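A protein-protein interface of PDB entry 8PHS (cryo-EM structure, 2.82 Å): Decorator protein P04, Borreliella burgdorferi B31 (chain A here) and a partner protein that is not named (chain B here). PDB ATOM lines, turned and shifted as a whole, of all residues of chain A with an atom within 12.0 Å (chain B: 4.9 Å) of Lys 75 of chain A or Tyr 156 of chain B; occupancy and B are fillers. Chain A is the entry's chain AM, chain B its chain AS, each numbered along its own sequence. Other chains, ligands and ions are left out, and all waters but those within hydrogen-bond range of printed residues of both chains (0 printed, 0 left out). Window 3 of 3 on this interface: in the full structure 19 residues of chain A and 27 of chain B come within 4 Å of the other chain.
The backbone carbonyl oxygen (O) of Arg 78 of chain B lies within hydrogen-bond range of the side-chain amide nitrogen (ND2) of Asn 154 of chain B, 3.4 Å away. O of Ile 72 of chain A sits close to OD1 of Asn 74 of chain A (3.1 Å).
Printed residues of chain B within 4 Å of Glu 73 of chain A: Arg 78. Printed residues of chain B within 4 Å of Asn 74 of chain A: Val 77 and Arg 78. Of chain B, only Val 77 (3.9 Å), Asn 154 (3.3 Å) and Tyr 156 (3.3 Å) come within 4 Å of Lys 75 of chain A. Of the printed residues of chain B, Val 76 of chain A touches Val 77, Met 161 and Pro 162. Ser 78 of chain A touches none of the printed residues of chain B. Printed residues of chain A within 4 Å of Arg 78 of chain B: Glu 73 (3.2 Å) and Asn 74 (3.3 Å). Of the printed residues of chain A, Asn 154 of chain B touches Lys 75. Tyr 156 of chain B touches just one residue of chain A: Lys 75. No residue of chain A comes within 4 Å of Gly 157 of chain B. Leu 158 of chain B touches none of the printed residues of chain A. No residue of chain A comes within 4 Å of Asn 160 of chain B. No residue of chain A comes within 4 Å of Leu 304 of chain B. Printed residues of chain A within 4 Å of Leu 305 of chain B: Phe 77 (3.5 Å).
The guanidinium group of Arg 78 of chain B is in salt-bridge range of the side-chain carboxylate of Glu 73 of chain A, at 3.7 Å. O of Asn 74 of chain A lies within hydrogen-bond range of N of Arg 78 of chain B (3.3 Å).
O of Asn 74 of chain A touches CG1 of Val 77 of chain B, at 3.3 Å. Val 77 of chain B touches Lys 75 of chain A. Lys 75 of chain A touches Asn 154 of chain B. Lys 75 of chain A touches Tyr 156 of chain B. Val 77 of chain B touches Val 76 of chain A. Met 161 of chain B touches Val 76 of chain A. CG1 of Val 76 of chain A touches O of Pro 162 of chain B, at 3.7 Å. CG2 of Val 77 of chain B touches CD1 of Phe 77 of chain A (3.5 Å). CE2 of Phe 77 of chain A touches CD2 of Leu 305 of chain B, at 3.5 Å.
Of the 14 printed residues of chain B, 7 touch a printed residue of chain A. Hydrophobic or aromatic side chains of chain B that line the printed part of chain A: Val 77, Tyr 156, Met 161 and Leu 305. Along chain B the printed residues that touch a printed residue of chain A span positions 77 to 305. Among the printed residues, Asp or Glu carboxylates within 4 Å of a Lys or Arg side-chain nitrogen of the other chain: Glu 73 of chain A with Arg 78 of chain B (3.7 Å).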
ATOM      1  N   ILE A  72       8.247 -21.061  10.477  1.00  0.00           N
ATOM      2  CA  ILE A  72       7.445 -20.041  11.140  1.00  0.00           C
ATOM      3  C   ILE A  72       8.332 -19.148  11.999  1.00  0.00           C
ATOM      4  O   ILE A  72       9.053 -19.630  12.871  1.00  0.00           O
ATOM      5  CB  ILE A  72       6.328 -20.677  11.988  1.00  0.00           C
ATOM      6  CG1 ILE A  72       5.385 -21.491  11.100  1.00  0.00           C
ATOM      7  CG2 ILE A  72       5.559 -19.607  12.748  1.00  0.00           C
ATOM      8  CD1 ILE A  72       4.250 -22.148  11.855  1.00  0.00           C
ATOM      9  N   GLU A  73       8.277 -17.844  11.740  1.00  0.00           N
ATOM     10  CA  GLU A  73       9.050 -16.893  12.527  1.00  0.00           C
ATOM     11  C   GLU A  73       8.531 -16.834  13.958  1.00  0.00           C
ATOM     12  O   GLU A  73       7.326 -16.926  14.204  1.00  0.00           O
ATOM     13  CB  GLU A  73       8.993 -15.504  11.892  1.00  0.00           C
ATOM     14  CG  GLU A  73       9.659 -15.412  10.530  1.00  0.00           C
ATOM     15  CD  GLU A  73       9.286 -14.146   9.784  1.00  0.00           C
ATOM     16  OE1 GLU A  73       8.455 -13.371  10.304  1.00  0.00           O
ATOM     17  OE2 GLU A  73       9.827 -13.922   8.681  1.00  0.00           O
ATOM     18  N   ASN A  74       9.453 -16.682  14.903  1.00  0.00           N
ATOM     19  CA  ASN A  74       9.126 -16.609  16.317  1.00  0.00           C
ATOM     20  C   ASN A  74       9.613 -15.287  16.893  1.00  0.00           C
ATOM     21  O   ASN A  74      10.662 -14.769  16.500  1.00  0.00           O
ATOM     22  CB  ASN A  74       9.753 -17.772  17.094  1.00  0.00           C
ATOM     23  CG  ASN A  74       9.201 -19.120  16.677  1.00  0.00           C
ATOM     24  OD1 ASN A  74       8.272 -19.202  15.874  1.00  0.00           O
ATOM     25  ND2 ASN A  74       9.774 -20.188  17.220  1.00  0.00           N
ATOM     26  N   LYS A  75       8.834 -14.739  17.827  1.00  0.00           N
ATOM     27  CA  LYS A  75       9.257 -13.532  18.524  1.00  0.00           C
ATOM     28  C   LYS A  75      10.352 -13.832  19.540  1.00  0.00           C
ATOM     29  O   LYS A  75      11.277 -13.032  19.714  1.00  0.00           O
ATOM     30  CB  LYS A  75       8.060 -12.872  19.209  1.00  0.00           C
ATOM     31  CG  LYS A  75       6.956 -12.448  18.258  1.00  0.00           C
ATOM     32  CD  LYS A  75       5.723 -11.990  19.018  1.00  0.00           C
ATOM     33  CE  LYS A  75       4.651 -11.474  18.073  1.00  0.00           C
ATOM     34  NZ  LYS A  75       3.428 -11.042  18.806  1.00  0.00           N
ATOM     35  N   VAL A  76      10.259 -14.976  20.219  1.00  0.00           N
ATOM     36  CA  VAL A  76      11.248 -15.399  21.200  1.00  0.00           C
ATOM     37  C   VAL A  76      11.605 -16.855  20.933  1.00  0.00           C
ATOM     38  O   VAL A  76      10.862 -17.594  20.286  1.00  0.00           O
ATOM     39  CB  VAL A  76      10.750 -15.226  22.652  1.00  0.00           C
ATOM     40  CG1 VAL A  76      10.452 -13.766  22.947  1.00  0.00           C
ATOM     41  CG2 VAL A  76       9.523 -16.087  22.897  1.00  0.00           C
ATOM     42  N   PHE A  77      12.764 -17.260  21.444  1.00  0.00           N
ATOM     43  CA  PHE A  77      13.199 -18.641  21.317  1.00  0.00           C
ATOM     44  C   PHE A  77      12.417 -19.541  22.265  1.00  0.00           C
ATOM     45  O   PHE A  77      11.954 -19.113  23.325  1.00  0.00           O
ATOM     46  CB  PHE A  77      14.695 -18.768  21.604  1.00  0.00           C
ATOM     47  CG  PHE A  77      15.561 -18.570  20.397  1.00  0.00           C
ATOM     48  CD1 PHE A  77      15.295 -19.249  19.222  1.00  0.00           C
ATOM     49  CD2 PHE A  77      16.645 -17.714  20.440  1.00  0.00           C
ATOM     50  CE1 PHE A  77      16.089 -19.069  18.108  1.00  0.00           C
ATOM     51  CE2 PHE A  77      17.445 -17.532  19.330  1.00  0.00           C
ATOM     52  CZ  PHE A  77      17.165 -18.209  18.163  1.00  0.00           C
ATOM     53  N   SER A  78      12.269 -20.802  21.866  1.00  0.00           N
ATOM     54  CA  SER A  78      11.620 -21.792  22.712  1.00  0.00           C
ATOM     55  C   SER A  78      12.592 -22.301  23.768  1.00  0.00           C
ATOM     56  O   SER A  78      13.784 -22.483  23.502  1.00  0.00           O
ATOM     57  CB  SER A  78      11.100 -22.957  21.871  1.00  0.00           C
ATOM     58  OG  SER A  78      12.169 -23.679  21.289  1.00  0.00           O
ATOM     59  N   SER A  79      12.075 -22.531  24.971  1.00  0.00           N
ATOM     60  CA  SER A  79      12.900 -22.986  26.086  1.00  0.00           C
ATOM     61  C   SER A  79      13.429 -24.396  25.850  1.00  0.00           C
ATOM     62  O   SER A  79      12.881 -25.150  25.046  1.00  0.00           O
ATOM     63  CB  SER A  79      12.105 -22.936  27.393  1.00  0.00           C
ATOM     64  OG  SER A  79      11.404 -21.711  27.515  1.00  0.00           O
ATOM     65  N   VAL B  77      14.126 -17.058  14.495  1.00  0.00           N
ATOM     66  CA  VAL B  77      13.544 -15.903  15.168  1.00  0.00           C
ATOM     67  C   VAL B  77      13.834 -14.663  14.333  1.00  0.00           C
ATOM     68  O   VAL B  77      14.966 -14.469  13.877  1.00  0.00           O
ATOM     69  CB  VAL B  77      14.096 -15.737  16.598  1.00  0.00           C
ATOM     70  CG1 VAL B  77      13.877 -14.320  17.098  1.00  0.00           C
ATOM     71  CG2 VAL B  77      13.444 -16.737  17.532  1.00  0.00           C
ATOM     72  N   ARG B  78      12.815 -13.833  14.131  1.00  0.00           N
ATOM     73  CA  ARG B  78      12.938 -12.607  13.356  1.00  0.00           C
ATOM     74  C   ARG B  78      13.120 -11.410  14.281  1.00  0.00           C
ATOM     75  O   ARG B  78      12.460 -11.306  15.318  1.00  0.00           O
ATOM     76  CB  ARG B  78      11.708 -12.398  12.472  1.00  0.00           C
ATOM     77  CG  ARG B  78      11.801 -11.195  11.551  1.00  0.00           C
ATOM     78  CD  ARG B  78      10.473 -10.911  10.873  1.00  0.00           C
ATOM     79  NE  ARG B  78      10.561  -9.777   9.962  1.00  0.00           N
ATOM     80  CZ  ARG B  78       9.549  -9.311   9.244  1.00  0.00           C
ATOM     81  NH1 ARG B  78       8.346  -9.860   9.308  1.00  0.00           N
ATOM     82  NH2 ARG B  78       9.747  -8.271   8.440  1.00  0.00           N
ATOM     83  N   GLY B 137      11.312  -0.735  26.329  1.00  0.00           N
ATOM     84  CA  GLY B 137      10.712  -1.169  25.087  1.00  0.00           C
ATOM     85  C   GLY B 137       9.814  -0.152  24.420  1.00  0.00           C
ATOM     86  O   GLY B 137       9.225  -0.462  23.376  1.00  0.00           O
ATOM     87  N   PRO B 153       6.474  -4.595  15.183  1.00  0.00           N
ATOM     88  CA  PRO B 153       6.525  -5.822  15.984  1.00  0.00           C
ATOM     89  C   PRO B 153       7.924  -6.419  15.959  1.00  0.00           C
ATOM     90  O   PRO B 153       8.790  -6.020  15.178  1.00  0.00           O
ATOM     91  CB  PRO B 153       5.506  -6.744  15.308  1.00  0.00           C
ATOM     92  CG  PRO B 153       4.673  -5.845  14.445  1.00  0.00           C
ATOM     93  CD  PRO B 153       5.574  -4.732  14.027  1.00  0.00           C
ATOM     94  N   ASN B 154       8.135  -7.392  16.846  1.00  0.00           N
ATOM     95  CA  ASN B 154       9.448  -8.006  17.051  1.00  0.00           C
ATOM     96  C   ASN B 154      10.487  -6.972  17.476  1.00  0.00           C
ATOM     97  O   ASN B 154      11.665  -7.076  17.130  1.00  0.00           O
ATOM     98  CB  ASN B 154       9.919  -8.761  15.804  1.00  0.00           C
ATOM     99  CG  ASN B 154       8.996  -9.902  15.432  1.00  0.00           C
ATOM    100  OD1 ASN B 154       8.008 -10.165  16.116  1.00  0.00           O
ATOM    101  ND2 ASN B 154       9.313 -10.586  14.341  1.00  0.00           N
ATOM    102  N   MET B 155      10.047  -5.962  18.229  1.00  0.00           N
ATOM    103  CA  MET B 155      10.916  -4.908  18.760  1.00  0.00           C
ATOM    104  C   MET B 155      10.490  -4.693  20.210  1.00  0.00           C
ATOM    105  O   MET B 155       9.564  -3.927  20.488  1.00  0.00           O
ATOM    106  CB  MET B 155      10.804  -3.629  17.942  1.00  0.00           C
ATOM    107  CG  MET B 155      11.764  -3.549  16.772  1.00  0.00           C
ATOM    108  SD  MET B 155      11.603  -2.000  15.867  1.00  0.00           S
ATOM    109  CE  MET B 155      12.621  -0.921  16.867  1.00  0.00           C
ATOM    110  N   TYR B 156      11.168  -5.372  21.130  1.00  0.00           N
ATOM    111  CA  TYR B 156      10.778  -5.373  22.530  1.00  0.00           C
ATOM    112  C   TYR B 156      11.965  -5.025  23.411  1.00  0.00           C
ATOM    113  O   TYR B 156      13.121  -5.264  23.053  1.00  0.00           O
ATOM    114  CB  TYR B 156      10.217  -6.734  22.959  1.00  0.00           C
ATOM    115  CG  TYR B 156       9.140  -7.276  22.051  1.00  0.00           C
ATOM    116  CD1 TYR B 156       7.858  -6.746  22.069  1.00  0.00           C
ATOM    117  CD2 TYR B 156       9.405  -8.322  21.179  1.00  0.00           C
ATOM    118  CE1 TYR B 156       6.872  -7.242  21.242  1.00  0.00           C
ATOM    119  CE2 TYR B 156       8.426  -8.823  20.349  1.00  0.00           C
ATOM    120  CZ  TYR B 156       7.162  -8.279  20.384  1.00  0.00           C
ATOM    121  OH  TYR B 156       6.183  -8.776  19.556  1.00  0.00           O
ATOM    122  N   GLY B 157      11.662  -4.450  24.575  1.00  0.00           N
ATOM    123  CA  GLY B 157      12.636  -4.261  25.623  1.00  0.00           C
ATOM    124  C   GLY B 157      12.570  -5.373  26.655  1.00  0.00           C
ATOM    125  O   GLY B 157      11.857  -6.366  26.504  1.00  0.00           O
ATOM    126  N   LEU B 158      13.337  -5.191  27.730  1.00  0.00           N
ATOM    127  CA  LEU B 158      13.345  -6.188  28.794  1.00  0.00           C
ATOM    128  C   LEU B 158      12.010  -6.245  29.526  1.00  0.00           C
ATOM    129  O   LEU B 158      11.648  -7.293  30.068  1.00  0.00           O
ATOM    130  CB  LEU B 158      14.475  -5.900  29.779  1.00  0.00           C
ATOM    131  CG  LEU B 158      15.897  -6.112  29.262  1.00  0.00           C
ATOM    132  CD1 LEU B 158      16.901  -5.412  30.160  1.00  0.00           C
ATOM    133  CD2 LEU B 158      16.209  -7.593  29.157  1.00  0.00           C
ATOM    134  N   ASN B 160       8.792  -5.456  28.249  1.00  0.00           N
ATOM    135  CA  ASN B 160       7.631  -5.850  27.460  1.00  0.00           C
ATOM    136  C   ASN B 160       7.907  -7.059  26.572  1.00  0.00           C
ATOM    137  O   ASN B 160       7.171  -7.295  25.610  1.00  0.00           O
ATOM    138  CB  ASN B 160       7.135  -4.677  26.615  1.00  0.00           C
ATOM    139  CG  ASN B 160       8.164  -4.202  25.611  1.00  0.00           C
ATOM    140  OD1 ASN B 160       9.332  -4.585  25.667  1.00  0.00           O
ATOM    141  ND2 ASN B 160       7.731  -3.366  24.675  1.00  0.00           N
ATOM    142  N   MET B 161       8.953  -7.822  26.867  1.00  0.00           N
ATOM    143  CA  MET B 161       9.238  -9.017  26.087  1.00  0.00           C
ATOM    144  C   MET B 161       8.121 -10.038  26.284  1.00  0.00           C
ATOM    145  O   MET B 161       7.770 -10.352  27.429  1.00  0.00           O
ATOM    146  CB  MET B 161      10.582  -9.616  26.496  1.00  0.00           C
ATOM    147  CG  MET B 161      11.022 -10.795  25.648  1.00  0.00           C
ATOM    148  SD  MET B 161      11.430 -10.330  23.956  1.00  0.00           S
ATOM    149  CE  MET B 161      13.064  -9.636  24.183  1.00  0.00           C
ATOM    150  N   PRO B 162       7.540 -10.568  25.213  1.00  0.00           N
ATOM    151  CA  PRO B 162       6.426 -11.508  25.360  1.00  0.00           C
ATOM    152  C   PRO B 162       6.888 -12.883  25.822  1.00  0.00           C
ATOM    153  O   PRO B 162       8.068 -13.231  25.764  1.00  0.00           O
ATOM    154  CB  PRO B 162       5.839 -11.573  23.947  1.00  0.00           C
ATOM    155  CG  PRO B 162       7.005 -11.305  23.066  1.00  0.00           C
ATOM    156  CD  PRO B 162       7.834 -10.284  23.798  1.00  0.00           C
ATOM    157  N   LEU B 304      16.859  -6.942  20.720  1.00  0.00           N
ATOM    158  CA  LEU B 304      16.837  -7.735  21.941  1.00  0.00           C
ATOM    159  C   LEU B 304      16.176  -9.079  21.665  1.00  0.00           C
ATOM    160  O   LEU B 304      15.080  -9.133  21.100  1.00  0.00           O
ATOM    161  CB  LEU B 304      16.102  -6.998  23.059  1.00  0.00           C
ATOM    162  CG  LEU B 304      16.288  -7.596  24.454  1.00  0.00           C
ATOM    163  CD1 LEU B 304      17.758  -7.609  24.836  1.00  0.00           C
ATOM    164  CD2 LEU B 304      15.475  -6.833  25.481  1.00  0.00           C
ATOM    165  N   LEU B 305      16.843 -10.163  22.064  1.00  0.00           N
ATOM    166  CA  LEU B 305      16.370 -11.515  21.817  1.00  0.00           C
ATOM    167  C   LEU B 305      16.432 -12.295  23.120  1.00  0.00           C
ATOM    168  O   LEU B 305      17.414 -12.192  23.858  1.00  0.00           O
ATOM    169  CB  LEU B 305      17.220 -12.188  20.736  1.00  0.00           C
ATOM    170  CG  LEU B 305      17.167 -13.703  20.573  1.00  0.00           C
ATOM    171  CD1 LEU B 305      15.776 -14.149  20.173  1.00  0.00           C
ATOM    172  CD2 LEU B 305      18.190 -14.131  19.539  1.00  0.00           C
